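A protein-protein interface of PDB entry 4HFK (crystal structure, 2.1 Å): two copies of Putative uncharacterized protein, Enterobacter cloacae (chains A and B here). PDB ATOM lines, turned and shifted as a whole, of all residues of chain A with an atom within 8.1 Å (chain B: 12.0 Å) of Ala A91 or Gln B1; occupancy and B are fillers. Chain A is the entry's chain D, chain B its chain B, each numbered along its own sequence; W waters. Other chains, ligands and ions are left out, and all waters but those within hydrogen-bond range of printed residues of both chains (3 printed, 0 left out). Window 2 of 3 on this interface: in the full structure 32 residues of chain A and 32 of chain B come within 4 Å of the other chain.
O of Gln B1 lies within hydrogen-bond range of NE2 of Gln A68, at 3.0 Å.
OG of Ser A89 is in hydrogen-bond range of O of Ile A86 (2.7 Å). The backbone NH (N) of Ile A92 lies within hydrogen-bond range of the side-chain hydroxyl (OG) of Ser A89 (3.3 Å).
Among the printed residues, merely in contact across the chains: Leu A65 with Gln B1, Leu A85 with Pro B4, Asn A88 with Phe B9, Ala A91 with Gln B1, Asn A88 with Pro B4, Leu A85 with Phe B9, Ser A89 with Pro B4 and Ile A86 with Leu B3.
Ala A58 touches none of the printed residues of chain B. No residue of chain B comes within 4 Å of Val A61. Ser A64 touches none of the printed residues of chain B. Of chain B, only Gln B1 (3.2 Å) comes within 4 Å of Leu A65. Leu A66 touches none of the printed residues of chain B. Printed residues of chain B within 4 Å of Leu A85: Pro B4 and Phe B9. Printed residues of chain B within 4 Å of Ile A86: Leu B3 (3.8 Å). Of chain B, only Gln B1 comes within 4 Å of Ala A91. No residue of chain B comes within 4 Å of Arg A93. No residue of chain B comes within 4 Å of Pro A94. Of the printed residues of chain A, Gln B1 touches Leu A65, Gln A68 and Ala A91. Of the printed residues of chain A, Leu B3 touches Ile A86. Printed residues of chain A within 4 Å of Pro B4: Leu A85, Asn A88 and Ser A89. The nearest printed residue of chain B that does not touch Ile A86 is Pro B4 (5.0 Å).
Hydrophobic or aromatic side chains of chain A that line the printed part of chain B: Leu A65, Leu A85, Ile A86 and Ala A91. Hydrophobic or aromatic side chains of chain B within 4 Å of the printed part of chain A: Leu B3, Pro B4 and Phe B9. Along chain B the printed residues that touch a printed residue of chain A span positions 1 to 9. Among the printed residues, 9 pairs touch across the chains. Among the printed residues, no Asp or Glu carboxylate lies within 4 Å of a Lys or Arg side-chain nitrogen of the other chain.
No position is printed for both chains. Of the 9 pairs that touch across the chains among the printed residues, none has its exchanged pair printed and touching as well.
Water W1 bridges OE1 of Gln A68 (2.6 Å) and N of Leu B3 (2.8 Å). Water W2 lies within hydrogen-bond range of O of Thr B2, N of Ala A91, OE1 of Gln B1 and N of Asp A90. Water W3 lies within hydrogen-bond range of the backbone NH of Asp A90 (2.8 Å) and the backbone carbonyl oxygen of Thr B2 (2.9 Å).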
ATOM      1  N   PHE A  15      14.124  10.216 -37.772  1.00  0.00           N
ATOM      2  CA  PHE A  15      13.558   9.551 -36.593  1.00  0.00           C
ATOM      3  C   PHE A  15      12.040   9.723 -36.532  1.00  0.00           C
ATOM      4  O   PHE A  15      11.315   8.777 -36.207  1.00  0.00           O
ATOM      5  CB  PHE A  15      14.196  10.064 -35.296  1.00  0.00           C
ATOM      6  CG  PHE A  15      13.842   9.235 -34.082  1.00  0.00           C
ATOM      7  CD1 PHE A  15      14.469   8.014 -33.854  1.00  0.00           C
ATOM      8  CD2 PHE A  15      12.886   9.674 -33.174  1.00  0.00           C
ATOM      9  CE1 PHE A  15      14.148   7.233 -32.741  1.00  0.00           C
ATOM     10  CE2 PHE A  15      12.551   8.899 -32.054  1.00  0.00           C
ATOM     11  CZ  PHE A  15      13.189   7.676 -31.839  1.00  0.00           C
ATOM     12  N   LYS A  57      12.657   2.352 -26.826  1.00  0.00           N
ATOM     13  CA  LYS A  57      11.838   3.172 -25.932  1.00  0.00           C
ATOM     14  C   LYS A  57      10.729   3.884 -26.696  1.00  0.00           C
ATOM     15  O   LYS A  57       9.597   3.986 -26.217  1.00  0.00           O
ATOM     16  CB  LYS A  57      12.709   4.189 -25.192  1.00  0.00           C
ATOM     17  CG  LYS A  57      13.601   3.564 -24.112  1.00  0.00           C
ATOM     18  CD  LYS A  57      14.616   4.583 -23.596  1.00  0.00           C
ATOM     19  CE  LYS A  57      15.457   4.029 -22.452  1.00  0.00           C
ATOM     20  NZ  LYS A  57      16.580   4.958 -22.130  1.00  0.00           N
ATOM     21  N   ALA A  58      11.050   4.364 -27.893  1.00  0.00           N
ATOM     22  CA  ALA A  58      10.048   5.047 -28.711  1.00  0.00           C
ATOM     23  C   ALA A  58       8.863   4.129 -29.035  1.00  0.00           C
ATOM     24  O   ALA A  58       7.704   4.559 -29.019  1.00  0.00           O
ATOM     25  CB  ALA A  58      10.681   5.595 -29.979  1.00  0.00           C
ATOM     26  N   VAL A  61       6.568   4.170 -26.214  1.00  0.00           N
ATOM     27  CA  VAL A  61       5.830   5.434 -26.214  1.00  0.00           C
ATOM     28  C   VAL A  61       4.706   5.383 -27.257  1.00  0.00           C
ATOM     29  O   VAL A  61       3.572   5.804 -26.996  1.00  0.00           O
ATOM     30  CB  VAL A  61       6.769   6.617 -26.479  1.00  0.00           C
ATOM     31  CG1 VAL A  61       5.979   7.902 -26.735  1.00  0.00           C
ATOM     32  CG2 VAL A  61       7.723   6.794 -25.291  1.00  0.00           C
ATOM     33  N   ILE A  62       5.024   4.831 -28.426  1.00  0.00           N
ATOM     34  CA  ILE A  62       4.055   4.685 -29.506  1.00  0.00           C
ATOM     35  C   ILE A  62       2.845   3.861 -29.056  1.00  0.00           C
ATOM     36  O   ILE A  62       1.698   4.273 -29.263  1.00  0.00           O
ATOM     37  CB  ILE A  62       4.700   4.023 -30.753  1.00  0.00           C
ATOM     38  CG1 ILE A  62       5.662   4.999 -31.451  1.00  0.00           C
ATOM     39  CG2 ILE A  62       3.626   3.570 -31.738  1.00  0.00           C
ATOM     40  CD1 ILE A  62       6.625   4.303 -32.459  1.00  0.00           C
ATOM     41  N   SER A  64       1.698   3.308 -26.101  1.00  0.00           N
ATOM     42  CA  SER A  64       0.941   4.099 -25.144  1.00  0.00           C
ATOM     43  C   SER A  64       0.115   5.211 -25.813  1.00  0.00           C
ATOM     44  O   SER A  64      -1.086   5.322 -25.575  1.00  0.00           O
ATOM     45  CB  SER A  64       1.890   4.683 -24.091  1.00  0.00           C
ATOM     46  OG  SER A  64       1.188   5.531 -23.203  1.00  0.00           O
ATOM     47  N   LEU A  65       0.744   6.021 -26.666  1.00  0.00           N
ATOM     48  CA  LEU A  65       0.037   7.156 -27.272  1.00  0.00           C
ATOM     49  C   LEU A  65      -1.042   6.749 -28.273  1.00  0.00           C
ATOM     50  O   LEU A  65      -2.003   7.479 -28.473  1.00  0.00           O
ATOM     51  CB  LEU A  65       1.013   8.144 -27.914  1.00  0.00           C
ATOM     52  CG  LEU A  65       1.935   8.904 -26.949  1.00  0.00           C
ATOM     53  CD1 LEU A  65       2.851   9.870 -27.698  1.00  0.00           C
ATOM     54  CD2 LEU A  65       1.135   9.646 -25.924  1.00  0.00           C
ATOM     55  N   LEU A  66      -0.894   5.585 -28.902  1.00  0.00           N
ATOM     56  CA  LEU A  66      -1.905   5.124 -29.853  1.00  0.00           C
ATOM     57  C   LEU A  66      -3.261   4.929 -29.179  1.00  0.00           C
ATOM     58  O   LEU A  66      -4.294   4.942 -29.843  1.00  0.00           O
ATOM     59  CB  LEU A  66      -1.460   3.826 -30.547  1.00  0.00           C
ATOM     60  CG  LEU A  66      -0.501   4.011 -31.724  1.00  0.00           C
ATOM     61  CD1 LEU A  66       0.024   2.655 -32.237  1.00  0.00           C
ATOM     62  CD2 LEU A  66      -1.207   4.786 -32.837  1.00  0.00           C
ATOM     63  N   GLN A  68      -4.694   6.998 -27.260  1.00  0.00           N
ATOM     64  CA  GLN A  68      -5.410   8.283 -27.264  1.00  0.00           C
ATOM     65  C   GLN A  68      -6.522   8.217 -28.295  1.00  0.00           C
ATOM     66  O   GLN A  68      -6.320   7.728 -29.415  1.00  0.00           O
ATOM     67  CB  GLN A  68      -4.494   9.460 -27.641  1.00  0.00           C
ATOM     68  CG  GLN A  68      -3.220   9.629 -26.814  1.00  0.00           C
ATOM     69  CD  GLN A  68      -3.386  10.577 -25.659  1.00  0.00           C
ATOM     70  OE1 GLN A  68      -3.988  11.645 -25.801  1.00  0.00           O
ATOM     71  NE2 GLN A  68      -2.850  10.198 -24.499  1.00  0.00           N
ATOM     72  N   LEU A  85       1.024  13.042 -35.429  1.00  0.00           N
ATOM     73  CA  LEU A  85       1.039  13.800 -34.180  1.00  0.00           C
ATOM     74  C   LEU A  85       1.945  13.099 -33.161  1.00  0.00           C
ATOM     75  O   LEU A  85       2.728  13.738 -32.454  1.00  0.00           O
ATOM     76  CB  LEU A  85      -0.384  13.949 -33.623  1.00  0.00           C
ATOM     77  CG  LEU A  85      -1.411  14.630 -34.536  1.00  0.00           C
ATOM     78  CD1 LEU A  85      -2.746  14.787 -33.817  1.00  0.00           C
ATOM     79  CD2 LEU A  85      -0.887  15.992 -34.990  1.00  0.00           C
ATOM     80  N   ILE A  86       1.847  11.777 -33.100  1.00  0.00           N
ATOM     81  CA  ILE A  86       2.719  10.999 -32.219  1.00  0.00           C
ATOM     82  C   ILE A  86       4.199  11.204 -32.569  1.00  0.00           C
ATOM     83  O   ILE A  86       5.016  11.473 -31.684  1.00  0.00           O
ATOM     84  CB  ILE A  86       2.357   9.507 -32.272  1.00  0.00           C
ATOM     85  CG1 ILE A  86       1.007   9.287 -31.577  1.00  0.00           C
ATOM     86  CG2 ILE A  86       3.428   8.662 -31.601  1.00  0.00           C
ATOM     87  CD1 ILE A  86       0.460   7.861 -31.719  1.00  0.00           C
ATOM     88  N   ALA A  87       4.544  11.087 -33.854  1.00  0.00           N
ATOM     89  CA  ALA A  87       5.929  11.277 -34.305  1.00  0.00           C
ATOM     90  C   ALA A  87       6.507  12.623 -33.838  1.00  0.00           C
ATOM     91  O   ALA A  87       7.712  12.757 -33.598  1.00  0.00           O
ATOM     92  CB  ALA A  87       5.999  11.173 -35.826  1.00  0.00           C
ATOM     93  N   ASN A  88       5.628  13.614 -33.725  1.00  0.00           N
ATOM     94  CA  ASN A  88       6.016  14.981 -33.369  1.00  0.00           C
ATOM     95  C   ASN A  88       5.661  15.378 -31.944  1.00  0.00           C
ATOM     96  O   ASN A  88       5.677  16.566 -31.610  1.00  0.00           O
ATOM     97  CB  ASN A  88       5.380  15.964 -34.354  1.00  0.00           C
ATOM     98  CG  ASN A  88       5.970  15.842 -35.728  1.00  0.00           C
ATOM     99  OD1 ASN A  88       7.020  16.424 -36.011  1.00  0.00           O
ATOM    100  ND2 ASN A  88       5.333  15.051 -36.586  1.00  0.00           N
ATOM    101  N   SER A  89       5.352  14.388 -31.102  1.00  0.00           N
ATOM    102  CA  SER A  89       4.936  14.649 -29.733  1.00  0.00           C
ATOM    103  C   SER A  89       6.104  14.946 -28.796  1.00  0.00           C
ATOM    104  O   SER A  89       7.247  14.546 -29.055  1.00  0.00           O
ATOM    105  CB  SER A  89       4.153  13.452 -29.178  1.00  0.00           C
ATOM    106  OG  SER A  89       4.975  12.294 -29.116  1.00  0.00           O
ATOM    107  N   ASP A  90       5.806  15.638 -27.702  1.00  0.00           N
ATOM    108  CA  ASP A  90       6.791  15.866 -26.653  1.00  0.00           C
ATOM    109  C   ASP A  90       7.289  14.549 -26.045  1.00  0.00           C
ATOM    110  O   ASP A  90       8.456  14.444 -25.664  1.00  0.00           O
ATOM    111  CB  ASP A  90       6.199  16.748 -25.555  1.00  0.00           C
ATOM    112  CG  ASP A  90       6.018  18.194 -26.000  1.00  0.00           C
ATOM    113  OD1 ASP A  90       6.449  18.545 -27.122  1.00  0.00           O
ATOM    114  OD2 ASP A  90       5.465  18.987 -25.212  1.00  0.00           O
ATOM    115  N   ALA A  91       6.408  13.552 -25.946  1.00  0.00           N
ATOM    116  CA  ALA A  91       6.793  12.269 -25.347  1.00  0.00           C
ATOM    117  C   ALA A  91       7.846  11.547 -26.183  1.00  0.00           C
ATOM    118  O   ALA A  91       8.658  10.782 -25.658  1.00  0.00           O
ATOM    119  CB  ALA A  91       5.567  11.375 -25.127  1.00  0.00           C
ATOM    120  N   ILE A  92       7.839  11.791 -27.488  1.00  0.00           N
ATOM    121  CA  ILE A  92       8.821  11.175 -28.371  1.00  0.00           C
ATOM    122  C   ILE A  92      10.110  12.016 -28.418  1.00  0.00           C
ATOM    123  O   ILE A  92      11.216  11.480 -28.586  1.00  0.00           O
ATOM    124  CB  ILE A  92       8.230  10.978 -29.783  1.00  0.00           C
ATOM    125  CG1 ILE A  92       7.239   9.803 -29.785  1.00  0.00           C
ATOM    126  CG2 ILE A  92       9.326  10.747 -30.819  1.00  0.00           C
ATOM    127  CD1 ILE A  92       7.916   8.424 -29.761  1.00  0.00           C
ATOM    128  N   ARG A  93       9.963  13.330 -28.238  1.00  0.00           N
ATOM    129  CA  ARG A  93      11.078  14.259 -28.444  1.00  0.00           C
ATOM    130  C   ARG A  93      12.423  13.889 -27.785  1.00  0.00           C
ATOM    131  O   ARG A  93      13.462  13.963 -28.441  1.00  0.00           O
ATOM    132  CB  ARG A  93      10.687  15.708 -28.091  1.00  0.00           C
ATOM    133  CG  ARG A  93      11.888  16.660 -28.117  1.00  0.00           C
ATOM    134  CD  ARG A  93      11.490  18.107 -28.364  1.00  0.00           C
ATOM    135  NE  ARG A  93      10.683  18.209 -29.568  1.00  0.00           N
ATOM    136  CZ  ARG A  93       9.369  18.388 -29.564  1.00  0.00           C
ATOM    137  NH1 ARG A  93       8.729  18.497 -28.412  1.00  0.00           N
ATOM    138  NH2 ARG A  93       8.701  18.444 -30.709  1.00  0.00           N
ATOM    139  N   PRO A  94      12.419  13.475 -26.505  1.00  0.00           N
ATOM    140  CA  PRO A  94      13.754  13.224 -25.948  1.00  0.00           C
ATOM    141  C   PRO A  94      14.485  12.037 -26.578  1.00  0.00           C
ATOM    142  O   PRO A  94      15.715  11.967 -26.476  1.00  0.00           O
ATOM    143  CB  PRO A  94      13.476  12.943 -24.472  1.00  0.00           C
ATOM    144  CG  PRO A  94      12.060  12.491 -24.426  1.00  0.00           C
ATOM    145  CD  PRO A  94      11.360  13.266 -25.502  1.00  0.00           C
ATOM    146  N   LEU A  95      13.753  11.133 -27.227  1.00  0.00           N
ATOM    147  CA  LEU A  95      14.380   9.992 -27.894  1.00  0.00           C
ATOM    148  C   LEU A  95      15.034  10.394 -29.221  1.00  0.00           C
ATOM    149  O   LEU A  95      15.633   9.561 -29.906  1.00  0.00           O
ATOM    150  CB  LEU A  95      13.360   8.868 -28.092  1.00  0.00           C
ATOM    151  CG  LEU A  95      12.730   8.511 -26.747  1.00  0.00           C
ATOM    152  CD1 LEU A  95      11.567   7.579 -26.920  1.00  0.00           C
ATOM    153  CD2 LEU A  95      13.759   7.903 -25.797  1.00  0.00           C
ATOM    154  N   LYS A  96      14.922  11.674 -29.576  1.00  0.00           N
ATOM    155  CA  LYS A  96      15.596  12.214 -30.757  1.00  0.00           C
ATOM    156  C   LYS A  96      17.053  12.572 -30.470  1.00  0.00           C
ATOM    157  O   LYS A  96      17.797  12.912 -31.383  1.00  0.00           O
ATOM    158  CB  LYS A  96      14.867  13.466 -31.267  1.00  0.00           C
ATOM    159  CG  LYS A  96      13.500  13.216 -31.912  1.00  0.00           C
ATOM    160  CD  LYS A  96      12.688  14.522 -31.949  1.00  0.00           C
ATOM    161  CE  LYS A  96      11.565  14.463 -32.961  1.00  0.00           C
ATOM    162  NZ  LYS A  96      10.870  15.772 -33.067  1.00  0.00           N
ATOM    163  N   GLN B   1       0.564  10.634 -22.782  1.00  0.00           N
ATOM    164  CA  GLN B   1       0.736  12.083 -22.732  1.00  0.00           C
ATOM    165  C   GLN B   1       0.034  12.773 -23.917  1.00  0.00           C
ATOM    166  O   GLN B   1      -0.524  12.115 -24.797  1.00  0.00           O
ATOM    167  CB  GLN B   1       2.225  12.447 -22.684  1.00  0.00           C
ATOM    168  CG  GLN B   1       2.524  13.729 -21.923  1.00  0.00           C
ATOM    169  CD  GLN B   1       3.808  14.397 -22.379  1.00  0.00           C
ATOM    170  OE1 GLN B   1       4.833  13.736 -22.579  1.00  0.00           O
ATOM    171  NE2 GLN B   1       3.758  15.717 -22.551  1.00  0.00           N
ATOM    172  N   THR B   2       0.063  14.102 -23.934  1.00  0.00           N
ATOM    173  CA  THR B   2      -0.739  14.869 -24.887  1.00  0.00           C
ATOM    174  C   THR B   2      -0.105  15.003 -26.281  1.00  0.00           C
ATOM    175  O   THR B   2       1.109  15.171 -26.429  1.00  0.00           O
ATOM    176  CB  THR B   2      -1.085  16.268 -24.329  1.00  0.00           C
ATOM    177  OG1 THR B   2       0.122  16.953 -23.977  1.00  0.00           O
ATOM    178  CG2 THR B   2      -1.970  16.150 -23.099  1.00  0.00           C
ATOM    179  N   LEU B   3      -0.947  14.928 -27.304  1.00  0.00           N
ATOM    180  CA  LEU B   3      -0.505  15.082 -28.680  1.00  0.00           C
ATOM    181  C   LEU B   3      -0.417  16.568 -29.034  1.00  0.00           C
ATOM    182  O   LEU B   3      -1.180  17.370 -28.499  1.00  0.00           O
ATOM    183  CB  LEU B   3      -1.482  14.358 -29.616  1.00  0.00           C
ATOM    184  CG  LEU B   3      -1.605  12.862 -29.317  1.00  0.00           C
ATOM    185  CD1 LEU B   3      -2.584  12.172 -30.269  1.00  0.00           C
ATOM    186  CD2 LEU B   3      -0.234  12.217 -29.410  1.00  0.00           C
ATOM    187  N   PRO B   4       0.510  16.937 -29.940  1.00  0.00           N
ATOM    188  CA  PRO B   4       0.633  18.330 -30.381  1.00  0.00           C
ATOM    189  C   PRO B   4      -0.580  18.770 -31.204  1.00  0.00           C
ATOM    190  O   PRO B   4      -1.214  17.953 -31.881  1.00  0.00           O
ATOM    191  CB  PRO B   4       1.882  18.305 -31.276  1.00  0.00           C
ATOM    192  CG  PRO B   4       1.952  16.896 -31.781  1.00  0.00           C
ATOM    193  CD  PRO B   4       1.491  16.061 -30.609  1.00  0.00           C
ATOM    194  N   ASP B   5      -0.906  20.052 -31.136  1.00  0.00           N
ATOM    195  CA  ASP B   5      -1.970  20.604 -31.970  1.00  0.00           C
ATOM    196  C   ASP B   5      -1.478  20.731 -33.415  1.00  0.00           C
ATOM    197  O   ASP B   5      -0.282  20.947 -33.644  1.00  0.00           O
ATOM    198  CB  ASP B   5      -2.366  21.982 -31.451  1.00  0.00           C
ATOM    199  CG  ASP B   5      -3.761  22.383 -31.882  1.00  0.00           C
ATOM    200  OD1 ASP B   5      -3.909  23.012 -32.962  1.00  0.00           O
ATOM    201  OD2 ASP B   5      -4.711  22.055 -31.135  1.00  0.00           O
ATOM    202  N   THR B   8       0.717  23.717 -34.355  1.00  0.00           N
ATOM    203  CA  THR B   8       2.127  23.795 -33.971  1.00  0.00           C
ATOM    204  C   THR B   8       3.083  23.390 -35.094  1.00  0.00           C
ATOM    205  O   THR B   8       4.301  23.499 -34.938  1.00  0.00           O
ATOM    206  CB  THR B   8       2.440  22.927 -32.735  1.00  0.00           C
ATOM    207  OG1 THR B   8       2.345  21.542 -33.086  1.00  0.00           O
ATOM    208  CG2 THR B   8       1.473  23.238 -31.590  1.00  0.00           C
ATOM    209  N   PHE B   9       2.546  22.902 -36.208  1.00  0.00           N
ATOM    210  CA  PHE B   9       3.376  22.560 -37.366  1.00  0.00           C
ATOM    211  C   PHE B   9       3.551  23.807 -38.232  1.00  0.00           C
ATOM    212  O   PHE B   9       2.739  24.730 -38.169  1.00  0.00           O
ATOM    213  CB  PHE B   9       2.715  21.452 -38.203  1.00  0.00           C
ATOM    214  CG  PHE B   9       2.644  20.112 -37.509  1.00  0.00           C
ATOM    215  CD1 PHE B   9       3.500  19.087 -37.875  1.00  0.00           C
ATOM    216  CD2 PHE B   9       1.729  19.883 -36.493  1.00  0.00           C
ATOM    217  CE1 PHE B   9       3.455  17.854 -37.237  1.00  0.00           C
ATOM    218  CE2 PHE B   9       1.676  18.645 -35.850  1.00  0.00           C
ATOM    219  CZ  PHE B   9       2.536  17.633 -36.229  1.00  0.00           C
HETATM  220  O   HOH W   1      -3.577  14.050 -26.665  1.00  0.00           O
HETATM  221  O   HOH W   2       3.502  14.064 -25.620  1.00  0.00           O
HETATM  222  O   HOH W   3       3.196  16.749 -27.763  1.00  0.00           O
